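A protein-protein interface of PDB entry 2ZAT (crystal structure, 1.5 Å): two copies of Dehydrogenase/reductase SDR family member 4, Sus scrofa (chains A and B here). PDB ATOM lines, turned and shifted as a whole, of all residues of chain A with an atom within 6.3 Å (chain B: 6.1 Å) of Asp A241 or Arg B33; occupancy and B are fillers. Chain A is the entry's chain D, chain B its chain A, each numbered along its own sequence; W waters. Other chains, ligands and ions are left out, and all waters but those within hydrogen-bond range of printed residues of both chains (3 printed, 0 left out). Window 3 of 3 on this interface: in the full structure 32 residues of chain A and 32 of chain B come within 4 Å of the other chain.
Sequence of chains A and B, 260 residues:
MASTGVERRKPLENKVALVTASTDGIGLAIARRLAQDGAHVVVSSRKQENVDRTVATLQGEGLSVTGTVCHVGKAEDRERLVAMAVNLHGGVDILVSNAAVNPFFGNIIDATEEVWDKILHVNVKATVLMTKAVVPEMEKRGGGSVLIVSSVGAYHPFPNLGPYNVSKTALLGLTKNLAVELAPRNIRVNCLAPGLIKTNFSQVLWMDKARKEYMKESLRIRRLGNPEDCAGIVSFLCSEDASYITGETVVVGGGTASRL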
ATOM      1  N   ARG A 188      -2.515  -5.328  -8.018  1.00  0.00           N
ATOM      2  CA  ARG A 188      -1.560  -4.279  -8.374  1.00  0.00           C
ATOM      3  C   ARG A 188      -0.586  -4.790  -9.377  1.00  0.00           C
ATOM      4  O   ARG A 188      -0.222  -5.977  -9.351  1.00  0.00           O
ATOM      5  CB  ARG A 188      -0.826  -3.809  -7.123  1.00  0.00           C
ATOM      6  CG  ARG A 188      -1.768  -3.168  -6.096  1.00  0.00           C
ATOM      7  CD  ARG A 188      -1.086  -2.546  -4.886  1.00  0.00           C
ATOM      8  NE  ARG A 188      -0.382  -3.593  -4.150  1.00  0.00           N
ATOM      9  CZ  ARG A 188       0.917  -3.848  -4.209  1.00  0.00           C
ATOM     10  NH1 ARG A 188       1.766  -3.115  -4.923  1.00  0.00           N
ATOM     11  NH2 ARG A 188       1.396  -4.888  -3.544  1.00  0.00           N
ATOM     12  N   PHE A 236       9.440  -5.413  -1.767  1.00  0.00           N
ATOM     13  CA  PHE A 236       8.629  -4.332  -1.225  1.00  0.00           C
ATOM     14  C   PHE A 236       7.358  -4.146  -2.047  1.00  0.00           C
ATOM     15  O   PHE A 236       6.255  -4.053  -1.493  1.00  0.00           O
ATOM     16  CB  PHE A 236       9.416  -3.006  -1.149  1.00  0.00           C
ATOM     17  CG  PHE A 236       8.535  -1.847  -0.821  1.00  0.00           C
ATOM     18  CD1 PHE A 236       8.088  -1.672   0.473  1.00  0.00           C
ATOM     19  CD2 PHE A 236       8.118  -0.986  -1.793  1.00  0.00           C
ATOM     20  CE1 PHE A 236       7.218  -0.632   0.772  1.00  0.00           C
ATOM     21  CE2 PHE A 236       7.246   0.058  -1.482  1.00  0.00           C
ATOM     22  CZ  PHE A 236       6.810   0.204  -0.213  1.00  0.00           C
ATOM     23  N   SER A 239       4.570  -6.557  -1.456  1.00  0.00           N
ATOM     24  CA  SER A 239       4.062  -6.569  -0.109  1.00  0.00           C
ATOM     25  C   SER A 239       2.853  -5.673   0.064  1.00  0.00           C
ATOM     26  O   SER A 239       2.637  -4.715  -0.696  1.00  0.00           O
ATOM     27  CB  SER A 239       5.160  -6.166   0.881  1.00  0.00           C
ATOM     28  OG  SER A 239       5.345  -4.766   0.947  1.00  0.00           O
ATOM     29  N   GLU A 240       2.092  -5.931   1.123  1.00  0.00           N
ATOM     30  CA  GLU A 240       0.912  -5.136   1.394  1.00  0.00           C
ATOM     31  C   GLU A 240       1.272  -3.705   1.827  1.00  0.00           C
ATOM     32  O   GLU A 240       0.448  -2.800   1.779  1.00  0.00           O
ATOM     33  CB  GLU A 240       0.002  -5.848   2.404  1.00  0.00           C
ATOM     34  CG  GLU A 240      -0.864  -6.943   1.775  1.00  0.00           C
ATOM     35  CD  GLU A 240      -1.704  -6.499   0.564  1.00  0.00           C
ATOM     36  OE1 GLU A 240      -2.083  -5.304   0.454  1.00  0.00           O
ATOM     37  OE2 GLU A 240      -1.993  -7.359  -0.305  1.00  0.00           O
ATOM     38  N   ASP A 241       2.512  -3.472   2.223  1.00  0.00           N
ATOM     39  CA  ASP A 241       2.974  -2.137   2.540  1.00  0.00           C
ATOM     40  C   ASP A 241       3.038  -1.208   1.311  1.00  0.00           C
ATOM     41  O   ASP A 241       3.191   0.021   1.422  1.00  0.00           O
ATOM     42  CB  ASP A 241       4.346  -2.250   3.166  1.00  0.00           C
ATOM     43  CG  ASP A 241       4.703  -1.069   3.985  1.00  0.00           C
ATOM     44  OD1 ASP A 241       3.803  -0.416   4.590  1.00  0.00           O
ATOM     45  OD2 ASP A 241       5.908  -0.764   4.121  1.00  0.00           O
ATOM     46  N   ALA A 242       2.963  -1.806   0.136  1.00  0.00           N
ATOM     47  CA  ALA A 242       2.958  -1.081  -1.125  1.00  0.00           C
ATOM     48  C   ALA A 242       1.542  -1.031  -1.716  1.00  0.00           C
ATOM     49  O   ALA A 242       1.358  -0.885  -2.943  1.00  0.00           O
ATOM     50  CB  ALA A 242       3.922  -1.757  -2.086  1.00  0.00           C
ATOM     51  N   SER A 243       0.516  -1.113  -0.861  1.00  0.00           N
ATOM     52  CA  SER A 243      -0.847  -1.217  -1.361  1.00  0.00           C
ATOM     53  C   SER A 243      -1.368  -0.020  -2.142  1.00  0.00           C
ATOM     54  O   SER A 243      -2.391  -0.177  -2.845  1.00  0.00           O
ATOM     55  CB  SER A 243      -1.819  -1.564  -0.236  1.00  0.00           C
ATOM     56  OG  SER A 243      -1.958  -0.479   0.647  1.00  0.00           O
ATOM     57  N   TYR A 244      -0.753   1.137  -2.031  1.00  0.00           N
ATOM     58  CA  TYR A 244      -1.157   2.322  -2.795  1.00  0.00           C
ATOM     59  C   TYR A 244      -0.210   2.587  -3.960  1.00  0.00           C
ATOM     60  O   TYR A 244      -0.183   3.679  -4.497  1.00  0.00           O
ATOM     61  CB  TYR A 244      -1.302   3.569  -1.900  1.00  0.00           C
ATOM     62  CG  TYR A 244      -2.336   4.575  -2.373  1.00  0.00           C
ATOM     63  CD1 TYR A 244      -3.656   4.199  -2.554  1.00  0.00           C
ATOM     64  CD2 TYR A 244      -1.995   5.874  -2.620  1.00  0.00           C
ATOM     65  CE1 TYR A 244      -4.600   5.111  -2.996  1.00  0.00           C
ATOM     66  CE2 TYR A 244      -2.937   6.797  -3.037  1.00  0.00           C
ATOM     67  CZ  TYR A 244      -4.233   6.402  -3.222  1.00  0.00           C
ATOM     68  OH  TYR A 244      -5.201   7.323  -3.663  1.00  0.00           O
ATOM     69  N   ILE A 245       0.575   1.594  -4.326  1.00  0.00           N
ATOM     70  CA  ILE A 245       1.482   1.696  -5.471  1.00  0.00           C
ATOM     71  C   ILE A 245       1.085   0.699  -6.550  1.00  0.00           C
ATOM     72  O   ILE A 245       1.167  -0.528  -6.348  1.00  0.00           O
ATOM     73  CB  ILE A 245       2.944   1.437  -5.058  1.00  0.00           C
ATOM     74  CG1 ILE A 245       3.347   2.364  -3.925  1.00  0.00           C
ATOM     75  CG2 ILE A 245       3.900   1.657  -6.261  1.00  0.00           C
ATOM     76  CD1 ILE A 245       4.757   2.155  -3.416  1.00  0.00           C
ATOM     77  N   LEU B  12      17.383   0.337   9.400  1.00  0.00           N
ATOM     78  CA  LEU B  12      18.019   1.630   9.598  1.00  0.00           C
ATOM     79  C   LEU B  12      18.652   1.722  10.982  1.00  0.00           C
ATOM     80  O   LEU B  12      18.854   2.788  11.497  1.00  0.00           O
ATOM     81  CB  LEU B  12      17.014   2.770   9.393  1.00  0.00           C
ATOM     82  CG  LEU B  12      16.262   2.747   8.063  1.00  0.00           C
ATOM     83  CD1 LEU B  12      15.299   3.893   8.083  1.00  0.00           C
ATOM     84  CD2 LEU B  12      17.170   2.851   6.861  1.00  0.00           C
ATOM     85  N   LEU B  28       5.104  13.209   9.302  1.00  0.00           N
ATOM     86  CA  LEU B  28       4.954  12.437  10.543  1.00  0.00           C
ATOM     87  C   LEU B  28       4.976  10.927  10.293  1.00  0.00           C
ATOM     88  O   LEU B  28       5.657  10.174  10.997  1.00  0.00           O
ATOM     89  CB  LEU B  28       3.668  12.848  11.277  1.00  0.00           C
ATOM     90  CG  LEU B  28       3.304  12.036  12.512  1.00  0.00           C
ATOM     91  CD1 LEU B  28       4.460  12.022  13.465  1.00  0.00           C
ATOM     92  CD2 LEU B  28       2.040  12.656  13.126  1.00  0.00           C
ATOM     93  N   ALA B  29       4.243  10.463   9.273  1.00  0.00           N
ATOM     94  CA  ALA B  29       4.228   9.037   8.981  1.00  0.00           C
ATOM     95  C   ALA B  29       5.621   8.546   8.608  1.00  0.00           C
ATOM     96  O   ALA B  29       6.022   7.475   8.992  1.00  0.00           O
ATOM     97  CB  ALA B  29       3.227   8.698   7.860  1.00  0.00           C
ATOM     98  N   ILE B  30       6.354   9.350   7.833  1.00  0.00           N
ATOM     99  CA  ILE B  30       7.734   9.018   7.472  1.00  0.00           C
ATOM    100  C   ILE B  30       8.628   8.951   8.721  1.00  0.00           C
ATOM    101  O   ILE B  30       9.335   7.986   8.925  1.00  0.00           O
ATOM    102  CB  ILE B  30       8.294  10.010   6.414  1.00  0.00           C
ATOM    103  CG1 ILE B  30       7.616   9.772   5.041  1.00  0.00           C
ATOM    104  CG2 ILE B  30       9.786   9.821   6.275  1.00  0.00           C
ATOM    105  CD1 ILE B  30       7.839  10.908   4.050  1.00  0.00           C
ATOM    106  N   ALA B  31       8.531   9.952   9.572  1.00  0.00           N
ATOM    107  CA  ALA B  31       9.362   9.990  10.777  1.00  0.00           C
ATOM    108  C   ALA B  31       9.076   8.785  11.669  1.00  0.00           C
ATOM    109  O   ALA B  31       9.999   8.106  12.139  1.00  0.00           O
ATOM    110  CB  ALA B  31       9.106  11.282  11.513  1.00  0.00           C
ATOM    111  N   ARG B  32       7.803   8.479  11.848  1.00  0.00           N
ATOM    112  CA  ARG B  32       7.408   7.308  12.606  1.00  0.00           C
ATOM    113  C   ARG B  32       8.019   6.028  12.036  1.00  0.00           C
ATOM    114  O   ARG B  32       8.581   5.205  12.748  1.00  0.00           O
ATOM    115  CB  ARG B  32       5.889   7.178  12.703  1.00  0.00           C
ATOM    116  CG  ARG B  32       5.433   5.925  13.386  1.00  0.00           C
ATOM    117  CD  ARG B  32       3.947   5.831  13.516  1.00  0.00           C
ATOM    118  NE  ARG B  32       3.453   6.682  14.588  1.00  0.00           N
ATOM    119  CZ  ARG B  32       2.640   7.720  14.461  1.00  0.00           C
ATOM    120  NH1 ARG B  32       2.215   8.153  13.281  1.00  0.00           N
ATOM    121  NH2 ARG B  32       2.236   8.383  15.544  1.00  0.00           N
ATOM    122  N   ARG B  33       7.892   5.815  10.728  1.00  0.00           N
ATOM    123  CA  ARG B  33       8.385   4.591  10.140  1.00  0.00           C
ATOM    124  C   ARG B  33       9.916   4.491  10.192  1.00  0.00           C
ATOM    125  O   ARG B  33      10.460   3.429  10.459  1.00  0.00           O
ATOM    126  CB  ARG B  33       7.912   4.456   8.689  1.00  0.00           C
ATOM    127  CG  ARG B  33       8.333   3.174   8.040  1.00  0.00           C
ATOM    128  CD  ARG B  33       7.710   1.897   8.662  1.00  0.00           C
ATOM    129  NE  ARG B  33       6.292   1.818   8.325  1.00  0.00           N
ATOM    130  CZ  ARG B  33       5.830   1.216   7.236  1.00  0.00           C
ATOM    131  NH1 ARG B  33       6.673   0.644   6.418  1.00  0.00           N
ATOM    132  NH2 ARG B  33       4.543   1.235   6.957  1.00  0.00           N
ATOM    133  N   LEU B  34      10.627   5.585   9.923  1.00  0.00           N
ATOM    134  CA  LEU B  34      12.076   5.553   9.987  1.00  0.00           C
ATOM    135  C   LEU B  34      12.511   5.105  11.391  1.00  0.00           C
ATOM    136  O   LEU B  34      13.427   4.311  11.524  1.00  0.00           O
ATOM    137  CB  LEU B  34      12.671   6.903   9.627  1.00  0.00           C
ATOM    138  CG  LEU B  34      12.500   7.424   8.195  1.00  0.00           C
ATOM    139  CD1 LEU B  34      13.161   8.756   8.021  1.00  0.00           C
ATOM    140  CD2 LEU B  34      13.045   6.468   7.153  1.00  0.00           C
ATOM    141  N   ALA B  35      11.844   5.647  12.399  1.00  0.00           N
ATOM    142  CA  ALA B  35      12.169   5.328  13.796  1.00  0.00           C
ATOM    143  C   ALA B  35      11.778   3.904  14.125  1.00  0.00           C
ATOM    144  O   ALA B  35      12.526   3.226  14.814  1.00  0.00           O
ATOM    145  CB  ALA B  35      11.508   6.313  14.736  1.00  0.00           C
ATOM    146  N   GLN B  36      10.630   3.429  13.641  1.00  0.00           N
ATOM    147  CA  GLN B  36      10.286   2.010  13.819  1.00  0.00           C
ATOM    148  C   GLN B  36      11.311   1.092  13.188  1.00  0.00           C
ATOM    149  O   GLN B  36      11.529  -0.040  13.643  1.00  0.00           O
ATOM    150  CB  GLN B  36       8.905   1.689  13.226  1.00  0.00           C
ATOM    151  CG  GLN B  36       7.766   2.306  13.978  1.00  0.00           C
ATOM    152  CD  GLN B  36       6.450   2.249  13.240  1.00  0.00           C
ATOM    153  OE1 GLN B  36       6.427   2.102  12.020  1.00  0.00           O
ATOM    154  NE2 GLN B  36       5.355   2.353  13.966  1.00  0.00           N
ATOM    155  N   ASP B  37      11.932   1.544  12.102  1.00  0.00           N
ATOM    156  CA  ASP B  37      12.932   0.784  11.384  1.00  0.00           C
ATOM    157  C   ASP B  37      14.353   0.952  11.936  1.00  0.00           C
ATOM    158  O   ASP B  37      15.293   0.448  11.351  1.00  0.00           O
ATOM    159  CB  ASP B  37      12.876   1.107   9.888  1.00  0.00           C
ATOM    160  CG  ASP B  37      11.649   0.524   9.217  1.00  0.00           C
ATOM    161  OD1 ASP B  37      10.938  -0.379   9.770  1.00  0.00           O
ATOM    162  OD2 ASP B  37      11.322   0.915   8.070  1.00  0.00           O
ATOM    163  N   GLY B  38      14.457   1.642  13.076  1.00  0.00           N
ATOM    164  CA  GLY B  38      15.676   1.681  13.867  1.00  0.00           C
ATOM    165  C   GLY B  38      16.425   2.982  13.886  1.00  0.00           C
ATOM    166  O   GLY B  38      17.428   3.118  14.595  1.00  0.00           O
ATOM    167  N   LEU B  63       9.993   5.107  20.521  1.00  0.00           N
ATOM    168  CA  LEU B  63      10.856   5.422  19.386  1.00  0.00           C
ATOM    169  C   LEU B  63      11.948   6.443  19.765  1.00  0.00           C
ATOM    170  O   LEU B  63      11.731   7.323  20.613  1.00  0.00           O
ATOM    171  CB  LEU B  63      10.002   5.942  18.219  1.00  0.00           C
ATOM    172  CG  LEU B  63       8.885   5.007  17.784  1.00  0.00           C
ATOM    173  CD1 LEU B  63       7.995   5.690  16.762  1.00  0.00           C
ATOM    174  CD2 LEU B  63       9.439   3.685  17.313  1.00  0.00           C
ATOM    175  N   GLU B 228       0.463   6.846   5.823  1.00  0.00           N
ATOM    176  CA  GLU B 228       1.291   5.659   5.994  1.00  0.00           C
ATOM    177  C   GLU B 228       1.542   4.915   4.680  1.00  0.00           C
ATOM    178  O   GLU B 228       2.492   4.155   4.577  1.00  0.00           O
ATOM    179  CB  GLU B 228       0.734   4.694   7.043  1.00  0.00           C
ATOM    180  CG  GLU B 228       1.768   3.632   7.415  1.00  0.00           C
ATOM    181  CD  GLU B 228       1.360   2.774   8.597  1.00  0.00           C
ATOM    182  OE1 GLU B 228       2.186   1.927   8.999  1.00  0.00           O
ATOM    183  OE2 GLU B 228       0.224   2.929   9.108  1.00  0.00           O
ATOM    184  N   ASP B 229       0.694   5.139   3.681  1.00  0.00           N
ATOM    185  CA  ASP B 229       0.891   4.530   2.367  1.00  0.00           C
ATOM    186  C   ASP B 229       2.160   5.011   1.706  1.00  0.00           C
ATOM    187  O   ASP B 229       2.629   4.362   0.770  1.00  0.00           O
ATOM    188  CB  ASP B 229      -0.232   4.891   1.416  1.00  0.00           C
ATOM    189  CG  ASP B 229      -1.525   4.212   1.717  1.00  0.00           C
ATOM    190  OD1 ASP B 229      -1.541   3.038   2.127  1.00  0.00           O
ATOM    191  OD2 ASP B 229      -2.590   4.815   1.489  1.00  0.00           O
ATOM    192  N   ALA B 231       5.022   5.765   3.614  1.00  0.00           N
ATOM    193  CA  ALA B 231       6.132   5.605   4.542  1.00  0.00           C
ATOM    194  C   ALA B 231       7.087   4.472   4.201  1.00  0.00           C
ATOM    195  O   ALA B 231       8.313   4.612   4.363  1.00  0.00           O
ATOM    196  CB  ALA B 231       5.546   5.417   5.940  1.00  0.00           C
ATOM    197  N   GLY B 232       6.553   3.345   3.746  1.00  0.00           N
ATOM    198  CA  GLY B 232       7.351   2.179   3.454  1.00  0.00           C
ATOM    199  C   GLY B 232       8.352   2.418   2.353  1.00  0.00           C
ATOM    200  O   GLY B 232       9.509   2.014   2.450  1.00  0.00           O
ATOM    201  N   ILE B 233       7.934   3.075   1.276  1.00  0.00           N
ATOM    202  CA  ILE B 233       8.860   3.294   0.177  1.00  0.00           C
ATOM    203  C   ILE B 233       9.979   4.248   0.608  1.00  0.00           C
ATOM    204  O   ILE B 233      11.108   4.111   0.174  1.00  0.00           O
ATOM    205  CB  ILE B 233       8.119   3.764  -1.113  1.00  0.00           C
ATOM    206  CG1 ILE B 233       9.061   3.878  -2.316  1.00  0.00           C
ATOM    207  CG2 ILE B 233       7.423   5.093  -0.910  1.00  0.00           C
ATOM    208  CD1 ILE B 233       9.631   2.564  -2.737  1.00  0.00           C
ATOM    209  N   SER B 235      11.224   4.625   3.685  1.00  0.00           N
ATOM    210  CA  SER B 235      12.147   3.862   4.508  1.00  0.00           C
ATOM    211  C   SER B 235      13.041   2.957   3.668  1.00  0.00           C
ATOM    212  O   SER B 235      14.248   2.897   3.870  1.00  0.00           O
ATOM    213  CB  SER B 235      11.376   3.051   5.510  1.00  0.00           C
ATOM    214  OG  SER B 235      12.284   2.399   6.381  1.00  0.00           O
HETATM  215  O   HOH W   1       0.103   0.878   2.058  1.00  0.00           O
HETATM  216  O   HOH W   2       3.982   2.227   3.357  1.00  0.00           O
HETATM  217  O   HOH W   3       1.520   2.001  -0.286  1.00  0.00           O
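OD2 of Asp A241 lies within salt-bridge range of NH1 of Arg B33.
N of Asp A241 sits close to OG of Ser A239 (3.4 Å). The backbone carbonyl oxygen (O) of Phe A236 lies within hydrogen-bond range of the side-chain hydroxyl (OG) of Ser A239 (2.7 Å). The guanidinium group (NH2) of Arg B33 lies within salt-bridge range of the side-chain carboxylate (OE1) of Glu B228.
Among the printed residues, pairs that only touch across the chains: Asp A241 with Gly B232 (3.3 Å), Phe A236 with Ile B233 (3.4 Å), Phe A236 with Gly B232 (3.6 Å), Tyr A244 with Asp B229 (3.7 Å) and Ser A243 with Asp B229 (3.8 Å).
Of the printed residues of chain B, Phe A236 touches Gly B232 (3.6 Å) and Ile B233 (3.4 Å). Asp A241 touches just these residues of chain B: Arg B33 and Gly B232. Printed residues of chain B within 4 Å of Ser A243: Asp B229. Printed residues of chain B within 4 Å of Tyr A244: Asp B229. Printed residues of chain A within 4 Å of Arg B33: Asp A241. Of the printed residues of chain A, Ile B233 touches Phe A236. The nearest residue of chain B that does not touch Asp A241 is Asp B229 (4.4 Å). The nearest printed residue of chain B that does not touch Tyr A244 is Glu B228 (7.3 Å).
Printed residues of chain B that touch a printed residue of chain A: Arg B33, Asp B229, Gly B232 and Ile B233. Hydrophobic or aromatic side chains of chain B that line the printed part of chain A: Ile B233. Printed residues of chain A that touch a printed residue of chain B: Phe A236, Asp A241, Ser A243 and Tyr A244. Among the printed residues, 6 pairs touch across the chains. Among the printed residues, Asp or Glu carboxylates within 4 Å of a Lys or Arg side-chain nitrogen of the other chain: Asp A241 with Arg B33 (2.8 Å).
No position is printed for both chains.
Water W1 lies within hydrogen-bond range of the side-chain carboxylate of Asp B229, the side-chain hydroxyl of Ser A243 and the backbone carbonyl oxygen of Asp A241. Water W2 lies within hydrogen-bond range of the backbone carbonyl oxygen (O) of Glu B228 (2.7 Å), the backbone NH (N) of Gly B232 (2.8 Å) and the side-chain carboxylate (OD1) of Asp A241 (2.9 Å). Water W3 lies within hydrogen-bond range of O of Asp B229 (2.8 Å), N of Tyr A244 (3.0 Å), O of Asp A241 (3.1 Å) and N of Ser A243 (3.3 Å).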
